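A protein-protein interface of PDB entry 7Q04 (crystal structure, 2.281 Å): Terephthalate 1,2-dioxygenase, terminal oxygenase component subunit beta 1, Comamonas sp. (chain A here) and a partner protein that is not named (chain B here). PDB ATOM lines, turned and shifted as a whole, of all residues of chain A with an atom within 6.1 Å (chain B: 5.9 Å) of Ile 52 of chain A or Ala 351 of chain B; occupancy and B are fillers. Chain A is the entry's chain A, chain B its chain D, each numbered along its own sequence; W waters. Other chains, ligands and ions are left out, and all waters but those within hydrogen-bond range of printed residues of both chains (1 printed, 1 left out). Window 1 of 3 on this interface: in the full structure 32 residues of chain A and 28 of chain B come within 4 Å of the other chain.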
ATOM      1  N   ARG A  37     -23.776  20.069  20.577  1.00  0.00           N
ATOM      2  CA  ARG A  37     -23.960  19.237  21.774  1.00  0.00           C
ATOM      3  C   ARG A  37     -25.461  19.105  22.046  1.00  0.00           C
ATOM      4  O   ARG A  37     -26.169  20.104  21.917  1.00  0.00           O
ATOM      5  CB  ARG A  37     -23.219  19.899  22.930  1.00  0.00           C
ATOM      6  CG  ARG A  37     -23.080  19.027  24.163  1.00  0.00           C
ATOM      7  CD  ARG A  37     -22.052  19.567  25.121  1.00  0.00           C
ATOM      8  NE  ARG A  37     -22.549  20.435  26.189  1.00  0.00           N
ATOM      9  CZ  ARG A  37     -22.203  21.724  26.335  1.00  0.00           C
ATOM     10  NH1 ARG A  37     -22.701  22.403  27.350  1.00  0.00           N
ATOM     11  NH2 ARG A  37     -21.405  22.335  25.466  1.00  0.00           N
ATOM     12  N   VAL A  38     -25.908  17.897  22.350  1.00  0.00           N
ATOM     13  CA  VAL A  38     -27.261  17.627  22.903  1.00  0.00           C
ATOM     14  C   VAL A  38     -27.054  17.275  24.379  1.00  0.00           C
ATOM     15  O   VAL A  38     -26.315  16.316  24.654  1.00  0.00           O
ATOM     16  CB  VAL A  38     -28.008  16.507  22.142  1.00  0.00           C
ATOM     17  CG1 VAL A  38     -29.304  16.186  22.843  1.00  0.00           C
ATOM     18  CG2 VAL A  38     -28.260  16.834  20.673  1.00  0.00           C
ATOM     19  N   THR A  39     -27.663  18.034  25.284  1.00  0.00           N
ATOM     20  CA  THR A  39     -27.549  17.814  26.744  1.00  0.00           C
ATOM     21  C   THR A  39     -28.916  18.102  27.376  1.00  0.00           C
ATOM     22  O   THR A  39     -29.933  18.089  26.633  1.00  0.00           O
ATOM     23  CB  THR A  39     -26.415  18.664  27.317  1.00  0.00           C
ATOM     24  OG1 THR A  39     -26.222  18.318  28.689  1.00  0.00           O
ATOM     25  CG2 THR A  39     -26.696  20.140  27.181  1.00  0.00           C
ATOM     26  N   ALA A  50     -20.489  16.830  29.024  1.00  0.00           N
ATOM     27  CA  ALA A  50     -20.779  15.690  28.142  1.00  0.00           C
ATOM     28  C   ALA A  50     -22.121  15.891  27.414  1.00  0.00           C
ATOM     29  O   ALA A  50     -23.023  16.560  27.931  1.00  0.00           O
ATOM     30  CB  ALA A  50     -20.769  14.440  28.966  1.00  0.00           C
ATOM     31  N   GLY A  51     -22.224  15.308  26.224  1.00  0.00           N
ATOM     32  CA  GLY A  51     -23.418  15.332  25.366  1.00  0.00           C
ATOM     33  C   GLY A  51     -23.742  13.949  24.850  1.00  0.00           C
ATOM     34  O   GLY A  51     -22.835  13.109  24.753  1.00  0.00           O
ATOM     35  N   ILE A  52     -25.016  13.736  24.541  1.00  0.00           N
ATOM     36  CA  ILE A  52     -25.533  12.556  23.803  1.00  0.00           C
ATOM     37  C   ILE A  52     -24.887  12.601  22.427  1.00  0.00           C
ATOM     38  O   ILE A  52     -24.530  11.523  21.878  1.00  0.00           O
ATOM     39  CB  ILE A  52     -27.076  12.616  23.748  1.00  0.00           C
ATOM     40  CG1 ILE A  52     -27.683  12.330  25.119  1.00  0.00           C
ATOM     41  CG2 ILE A  52     -27.668  11.676  22.694  1.00  0.00           C
ATOM     42  CD1 ILE A  52     -29.141  12.653  25.173  1.00  0.00           C
ATOM     43  N   VAL A  53     -24.807  13.826  21.902  1.00  0.00           N
ATOM     44  CA  VAL A  53     -23.987  14.216  20.726  1.00  0.00           C
ATOM     45  C   VAL A  53     -23.015  15.296  21.216  1.00  0.00           C
ATOM     46  O   VAL A  53     -23.462  16.164  21.991  1.00  0.00           O
ATOM     47  CB  VAL A  53     -24.841  14.707  19.545  1.00  0.00           C
ATOM     48  CG1 VAL A  53     -23.986  15.094  18.369  1.00  0.00           C
ATOM     49  CG2 VAL A  53     -25.828  13.661  19.088  1.00  0.00           C
ATOM     50  N   TRP A  54     -21.754  15.217  20.779  1.00  0.00           N
ATOM     51  CA  TRP A  54     -20.629  16.123  21.154  1.00  0.00           C
ATOM     52  C   TRP A  54     -19.690  16.235  19.958  1.00  0.00           C
ATOM     53  O   TRP A  54     -19.115  15.195  19.551  1.00  0.00           O
ATOM     54  CB  TRP A  54     -19.854  15.610  22.378  1.00  0.00           C
ATOM     55  CG  TRP A  54     -19.047  16.668  23.057  1.00  0.00           C
ATOM     56  CD1 TRP A  54     -19.394  17.356  24.186  1.00  0.00           C
ATOM     57  CD2 TRP A  54     -17.739  17.148  22.685  1.00  0.00           C
ATOM     58  NE1 TRP A  54     -18.412  18.251  24.521  1.00  0.00           N
ATOM     59  CE2 TRP A  54     -17.379  18.136  23.627  1.00  0.00           C
ATOM     60  CE3 TRP A  54     -16.855  16.854  21.647  1.00  0.00           C
ATOM     61  CZ2 TRP A  54     -16.178  18.838  23.557  1.00  0.00           C
ATOM     62  CZ3 TRP A  54     -15.665  17.540  21.581  1.00  0.00           C
ATOM     63  CH2 TRP A  54     -15.325  18.517  22.526  1.00  0.00           C
ATOM     64  N   ARG A  64     -21.005  11.697  11.849  1.00  0.00           N
ATOM     65  CA  ARG A  64     -22.213  11.231  12.578  1.00  0.00           C
ATOM     66  C   ARG A  64     -23.277  10.839  11.548  1.00  0.00           C
ATOM     67  O   ARG A  64     -23.959   9.802  11.733  1.00  0.00           O
ATOM     68  CB  ARG A  64     -22.753  12.290  13.548  1.00  0.00           C
ATOM     69  CG  ARG A  64     -24.055  11.869  14.220  1.00  0.00           C
ATOM     70  CD  ARG A  64     -24.322  12.571  15.521  1.00  0.00           C
ATOM     71  NE  ARG A  64     -23.484  12.065  16.596  1.00  0.00           N
ATOM     72  CZ  ARG A  64     -23.697  10.952  17.276  1.00  0.00           C
ATOM     73  NH1 ARG A  64     -24.738  10.187  17.021  1.00  0.00           N
ATOM     74  NH2 ARG A  64     -22.876  10.621  18.254  1.00  0.00           N
ATOM     75  N   ASN A  72     -25.455   2.639  11.574  1.00  0.00           N
ATOM     76  CA  ASN A  72     -26.497   2.583  12.630  1.00  0.00           C
ATOM     77  C   ASN A  72     -27.765   1.923  12.052  1.00  0.00           C
ATOM     78  O   ASN A  72     -28.163   2.226  10.888  1.00  0.00           O
ATOM     79  CB  ASN A  72     -26.740   3.968  13.242  1.00  0.00           C
ATOM     80  CG  ASN A  72     -25.533   4.519  13.976  1.00  0.00           C
ATOM     81  OD1 ASN A  72     -24.900   3.769  14.725  1.00  0.00           O
ATOM     82  ND2 ASN A  72     -25.274   5.818  13.840  1.00  0.00           N
ATOM     83  N   THR A 146     -34.541  10.457  27.314  1.00  0.00           N
ATOM     84  CA  THR A 146     -34.671  10.178  25.861  1.00  0.00           C
ATOM     85  C   THR A 146     -35.405   8.845  25.702  1.00  0.00           C
ATOM     86  O   THR A 146     -35.010   7.851  26.335  1.00  0.00           O
ATOM     87  CB  THR A 146     -33.310  10.175  25.163  1.00  0.00           C
ATOM     88  OG1 THR A 146     -32.720  11.485  25.275  1.00  0.00           O
ATOM     89  CG2 THR A 146     -33.436   9.824  23.706  1.00  0.00           C
ATOM     90  N   LEU A 149     -34.021   5.756  22.058  1.00  0.00           N
ATOM     91  CA  LEU A 149     -32.692   6.130  21.539  1.00  0.00           C
ATOM     92  C   LEU A 149     -32.825   7.471  20.844  1.00  0.00           C
ATOM     93  O   LEU A 149     -33.948   7.906  20.667  1.00  0.00           O
ATOM     94  CB  LEU A 149     -32.185   5.066  20.562  1.00  0.00           C
ATOM     95  CG  LEU A 149     -33.086   4.792  19.341  1.00  0.00           C
ATOM     96  CD1 LEU A 149     -32.979   5.877  18.271  1.00  0.00           C
ATOM     97  CD2 LEU A 149     -32.757   3.441  18.721  1.00  0.00           C
ATOM     98  N   MET A 150     -31.690   8.064  20.481  1.00  0.00           N
ATOM     99  CA  MET A 150     -31.624   9.289  19.652  1.00  0.00           C
ATOM    100  C   MET A 150     -30.799   8.965  18.418  1.00  0.00           C
ATOM    101  O   MET A 150     -29.602   8.738  18.583  1.00  0.00           O
ATOM    102  CB  MET A 150     -31.016  10.490  20.388  1.00  0.00           C
ATOM    103  CG  MET A 150     -31.242  11.768  19.626  1.00  0.00           C
ATOM    104  SD  MET A 150     -30.698  13.245  20.481  1.00  0.00           S
ATOM    105  CE  MET A 150     -31.885  13.323  21.801  1.00  0.00           C
ATOM    106  N   ALA A 151     -31.442   8.904  17.249  1.00  0.00           N
ATOM    107  CA  ALA A 151     -30.770   8.584  15.969  1.00  0.00           C
ATOM    108  C   ALA A 151     -30.403   9.891  15.280  1.00  0.00           C
ATOM    109  O   ALA A 151     -29.286  10.090  14.910  1.00  0.00           O
ATOM    110  CB  ALA A 151     -31.637   7.720  15.083  1.00  0.00           C
ATOM    111  N   PHE B 192     -27.507  11.015  31.600  1.00  0.00           N
ATOM    112  CA  PHE B 192     -28.608  10.864  30.616  1.00  0.00           C
ATOM    113  C   PHE B 192     -29.411   9.621  30.984  1.00  0.00           C
ATOM    114  O   PHE B 192     -28.835   8.645  31.465  1.00  0.00           O
ATOM    115  CB  PHE B 192     -28.083  10.810  29.186  1.00  0.00           C
ATOM    116  CG  PHE B 192     -27.283  12.032  28.794  1.00  0.00           C
ATOM    117  CD1 PHE B 192     -27.914  13.224  28.454  1.00  0.00           C
ATOM    118  CD2 PHE B 192     -25.899  12.022  28.849  1.00  0.00           C
ATOM    119  CE1 PHE B 192     -27.179  14.359  28.138  1.00  0.00           C
ATOM    120  CE2 PHE B 192     -25.164  13.160  28.530  1.00  0.00           C
ATOM    121  CZ  PHE B 192     -25.803  14.331  28.172  1.00  0.00           C
ATOM    122  N   TYR B 327     -21.850   9.274  33.118  1.00  0.00           N
ATOM    123  CA  TYR B 327     -20.581   9.372  32.348  1.00  0.00           C
ATOM    124  C   TYR B 327     -19.482   9.836  33.325  1.00  0.00           C
ATOM    125  O   TYR B 327     -19.787  10.700  34.174  1.00  0.00           O
ATOM    126  CB  TYR B 327     -20.688  10.365  31.185  1.00  0.00           C
ATOM    127  CG  TYR B 327     -21.553   9.993  29.998  1.00  0.00           C
ATOM    128  CD1 TYR B 327     -22.496   8.987  30.030  1.00  0.00           C
ATOM    129  CD2 TYR B 327     -21.451  10.710  28.817  1.00  0.00           C
ATOM    130  CE1 TYR B 327     -23.297   8.693  28.931  1.00  0.00           C
ATOM    131  CE2 TYR B 327     -22.252  10.445  27.717  1.00  0.00           C
ATOM    132  CZ  TYR B 327     -23.199   9.444  27.778  1.00  0.00           C
ATOM    133  OH  TYR B 327     -23.975   9.180  26.680  1.00  0.00           O
ATOM    134  N   ALA B 345     -17.393   9.718  24.023  1.00  0.00           N
ATOM    135  CA  ALA B 345     -18.771   9.539  24.547  1.00  0.00           C
ATOM    136  C   ALA B 345     -19.779   9.345  23.388  1.00  0.00           C
ATOM    137  O   ALA B 345     -20.854   8.757  23.634  1.00  0.00           O
ATOM    138  CB  ALA B 345     -19.158  10.709  25.407  1.00  0.00           C
ATOM    139  N   ASN B 346     -19.480   9.849  22.183  1.00  0.00           N
ATOM    140  CA  ASN B 346     -20.330   9.672  20.985  1.00  0.00           C
ATOM    141  C   ASN B 346     -20.510   8.183  20.695  1.00  0.00           C
ATOM    142  O   ASN B 346     -21.398   7.860  19.899  1.00  0.00           O
ATOM    143  CB  ASN B 346     -19.751  10.372  19.762  1.00  0.00           C
ATOM    144  CG  ASN B 346     -19.905  11.870  19.848  1.00  0.00           C
ATOM    145  OD1 ASN B 346     -20.994  12.375  19.622  1.00  0.00           O
ATOM    146  ND2 ASN B 346     -18.837  12.589  20.144  1.00  0.00           N
ATOM    147  N   LEU B 347     -19.695   7.311  21.292  1.00  0.00           N
ATOM    148  CA  LEU B 347     -19.757   5.849  21.063  1.00  0.00           C
ATOM    149  C   LEU B 347     -20.854   5.247  21.914  1.00  0.00           C
ATOM    150  O   LEU B 347     -21.349   4.198  21.530  1.00  0.00           O
ATOM    151  CB  LEU B 347     -18.452   5.189  21.482  1.00  0.00           C
ATOM    152  CG  LEU B 347     -17.225   5.544  20.680  1.00  0.00           C
ATOM    153  CD1 LEU B 347     -16.050   4.775  21.272  1.00  0.00           C
ATOM    154  CD2 LEU B 347     -17.432   5.206  19.218  1.00  0.00           C
ATOM    155  N   ILE B 348     -21.195   5.900  23.026  1.00  0.00           N
ATOM    156  CA  ILE B 348     -22.073   5.331  24.087  1.00  0.00           C
ATOM    157  C   ILE B 348     -23.316   6.202  24.286  1.00  0.00           C
ATOM    158  O   ILE B 348     -23.403   7.295  23.724  1.00  0.00           O
ATOM    159  CB  ILE B 348     -21.292   5.198  25.413  1.00  0.00           C
ATOM    160  CG1 ILE B 348     -20.897   6.568  25.977  1.00  0.00           C
ATOM    161  CG2 ILE B 348     -20.093   4.283  25.239  1.00  0.00           C
ATOM    162  CD1 ILE B 348     -20.719   6.535  27.466  1.00  0.00           C
ATOM    163  N   GLY B 349     -24.223   5.720  25.124  1.00  0.00           N
ATOM    164  CA  GLY B 349     -25.475   6.406  25.467  1.00  0.00           C
ATOM    165  C   GLY B 349     -26.504   6.342  24.349  1.00  0.00           C
ATOM    166  O   GLY B 349     -26.388   5.559  23.396  1.00  0.00           O
ATOM    167  N   PRO B 350     -27.555   7.183  24.478  1.00  0.00           N
ATOM    168  CA  PRO B 350     -28.731   7.099  23.616  1.00  0.00           C
ATOM    169  C   PRO B 350     -28.466   7.222  22.119  1.00  0.00           C
ATOM    170  O   PRO B 350     -29.238   6.654  21.400  1.00  0.00           O
ATOM    171  CB  PRO B 350     -29.596   8.260  24.093  1.00  0.00           C
ATOM    172  CG  PRO B 350     -29.175   8.426  25.527  1.00  0.00           C
ATOM    173  CD  PRO B 350     -27.683   8.226  25.505  1.00  0.00           C
ATOM    174  N   ALA B 351     -27.414   7.937  21.710  1.00  0.00           N
ATOM    175  CA  ALA B 351     -27.026   8.159  20.280  1.00  0.00           C
ATOM    176  C   ALA B 351     -25.682   7.485  19.940  1.00  0.00           C
ATOM    177  O   ALA B 351     -25.105   7.814  18.897  1.00  0.00           O
ATOM    178  CB  ALA B 351     -26.994   9.642  19.982  1.00  0.00           C
ATOM    179  N   GLY B 352     -25.209   6.556  20.768  1.00  0.00           N
ATOM    180  CA  GLY B 352     -23.884   5.939  20.615  1.00  0.00           C
ATOM    181  C   GLY B 352     -23.684   5.233  19.282  1.00  0.00           C
ATOM    182  O   GLY B 352     -24.524   4.383  18.909  1.00  0.00           O
ATOM    183  N   PHE B 353     -22.580   5.507  18.597  1.00  0.00           N
ATOM    184  CA  PHE B 353     -22.192   4.747  17.382  1.00  0.00           C
ATOM    185  C   PHE B 353     -22.243   3.247  17.712  1.00  0.00           C
ATOM    186  O   PHE B 353     -22.765   2.478  16.895  1.00  0.00           O
ATOM    187  CB  PHE B 353     -20.837   5.213  16.866  1.00  0.00           C
ATOM    188  CG  PHE B 353     -20.806   6.669  16.463  1.00  0.00           C
ATOM    189  CD1 PHE B 353     -21.828   7.227  15.710  1.00  0.00           C
ATOM    190  CD2 PHE B 353     -19.733   7.488  16.801  1.00  0.00           C
ATOM    191  CE1 PHE B 353     -21.778   8.559  15.317  1.00  0.00           C
ATOM    192  CE2 PHE B 353     -19.697   8.822  16.427  1.00  0.00           C
ATOM    193  CZ  PHE B 353     -20.722   9.357  15.690  1.00  0.00           C
ATOM    194  N   SER B 355     -23.730   1.919  20.883  1.00  0.00           N
ATOM    195  CA  SER B 355     -24.815   1.490  21.800  1.00  0.00           C
ATOM    196  C   SER B 355     -26.223   1.942  21.351  1.00  0.00           C
ATOM    197  O   SER B 355     -27.182   1.602  22.064  1.00  0.00           O
ATOM    198  CB  SER B 355     -24.503   1.955  23.203  1.00  0.00           C
ATOM    199  OG  SER B 355     -24.404   3.357  23.221  1.00  0.00           O
ATOM    200  N   MET B 356     -26.380   2.704  20.267  1.00  0.00           N
ATOM    201  CA  MET B 356     -27.705   3.214  19.808  1.00  0.00           C
ATOM    202  C   MET B 356     -28.700   2.051  19.747  1.00  0.00           C
ATOM    203  O   MET B 356     -29.762   2.170  20.399  1.00  0.00           O
ATOM    204  CB  MET B 356     -27.578   3.852  18.420  1.00  0.00           C
ATOM    205  CG  MET B 356     -28.737   4.700  18.038  1.00  0.00           C
ATOM    206  SD  MET B 356     -28.575   5.393  16.371  1.00  0.00           S
ATOM    207  CE  MET B 356     -27.202   6.530  16.492  1.00  0.00           C
HETATM  208  O   HOH W   1     -25.373   9.298  23.258  1.00  0.00           O
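Water W1 lies within hydrogen-bond range of O of Ile 52 of chain A, O of Ile 348 of chain B and N of Ala 351 of chain B.
The backbone NH (N) of Met 150 of chain A sits at hydrogen-bond distance from the backbone carbonyl oxygen (O) of Pro 350 of chain B. NH2 of Arg 64 of chain A lies within hydrogen-bond range of OD1 of Asn 346 of chain B (2.9 Å). The backbone carbonyl oxygen (O) of Trp 54 of chain A lies within hydrogen-bond range of the side-chain amide nitrogen (ND2) of Asn 346 of chain B. The backbone carbonyl oxygen (O) of Ala 351 of chain B is in hydrogen-bond range of the guanidinium group (NH1) of Arg 64 of chain A, at 3.0 Å. OD1 of Asn 72 of chain A lies close to O of Phe 353 of chain B, 3.3 Å away.
The backbone NH of Phe 353 of chain B lies within hydrogen-bond range of the backbone carbonyl oxygen of Asn 346 of chain B (2.9 Å). The backbone NH of Ile 52 of chain A lies within hydrogen-bond range of the backbone carbonyl oxygen of Val 38 of chain A, at 2.9 Å. N of Phe 353 of chain B sits at hydrogen-bond distance from O of Leu 347 of chain B. The backbone NH (N) of Val 38 of chain A sits at hydrogen-bond distance from the backbone carbonyl oxygen (O) of Val 53 of chain A, at 3.0 Å.
Of the 14 printed residues of chain A, 11 touch a printed residue of chain B. Hydrophobic or aromatic side chains of chain A that line the printed part of chain B: Ala 50, Ile 52, Trp 54 and Leu 149. Of the 13 printed residues of chain B, 7 touch a printed residue of chain A. Printed residues of chain B that touch a printed residue of chain A: Phe 192, Tyr 327, Asn 346, Pro 350, Ala 351, Phe 353 and Met 356. Among the printed residues, 19 pairs touch across the chains. Among the printed residues, no Asp or Glu carboxylate lies within 4 Å of a Lys or Arg side-chain nitrogen of the other chain.
CE1 of Phe 192 of chain B touches CA of Thr 39 of chain A (3.7 Å). O of Ala 50 of chain A touches CZ of Phe 192 of chain B, at 3.6 Å. CD2 of Tyr 327 of chain B touches CB of Ala 50 of chain A (3.8 Å). Phe 192 of chain B touches Ile 52 of chain A. CG2 of Ile 52 of chain A touches CB of Ala 351 of chain B, at 3.5 Å. Arg 64 of chain A touches Phe 353 of chain B. Asn 72 of chain A touches Met 356 of chain B. Pro 350 of chain B touches Leu 149 of chain A (O to CB, 3.5 Å). Leu 149 of chain A touches Met 356 of chain B. Met 150 of chain A touches Met 356 of chain B (O to CE, 3.9 Å).
Ile 52 of chain A touches just these residues of chain B: Phe 192 (3.5 Å) and Ala 351 (3.5 Å). Of the printed residues of chain A, Ala 351 of chain B touches Ile 52 (3.5 Å), Arg 64 (3.0 Å) and Met 150 (3.1 Å). Of the printed residues of chain A, Met 356 of chain B touches Asn 72, Leu 149, Met 150 and Ala 151. Printed residues of chain B within 4 Å of Asn 72 of chain A: Phe 353 and Met 356. Of the printed residues of chain B, Ala 151 of chain A touches Met 356 (3.9 Å). Printed residues of chain A within 4 Å of Asn 346 of chain B: Val 53, Trp 54 and Arg 64. Of the printed residues of chain A, Pro 350 of chain B touches Leu 149 (3.5 Å) and Met 150 (3.0 Å). Val 38 of chain A touches none of the printed residues of chain B. The nearest residue of chain B that does not touch Ile 52 of chain A is Pro 350 of chain B (4.1 Å). The nearest residue of chain A that does not touch Ala 351 of chain B is Val 53 of chain A (4.3 Å).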
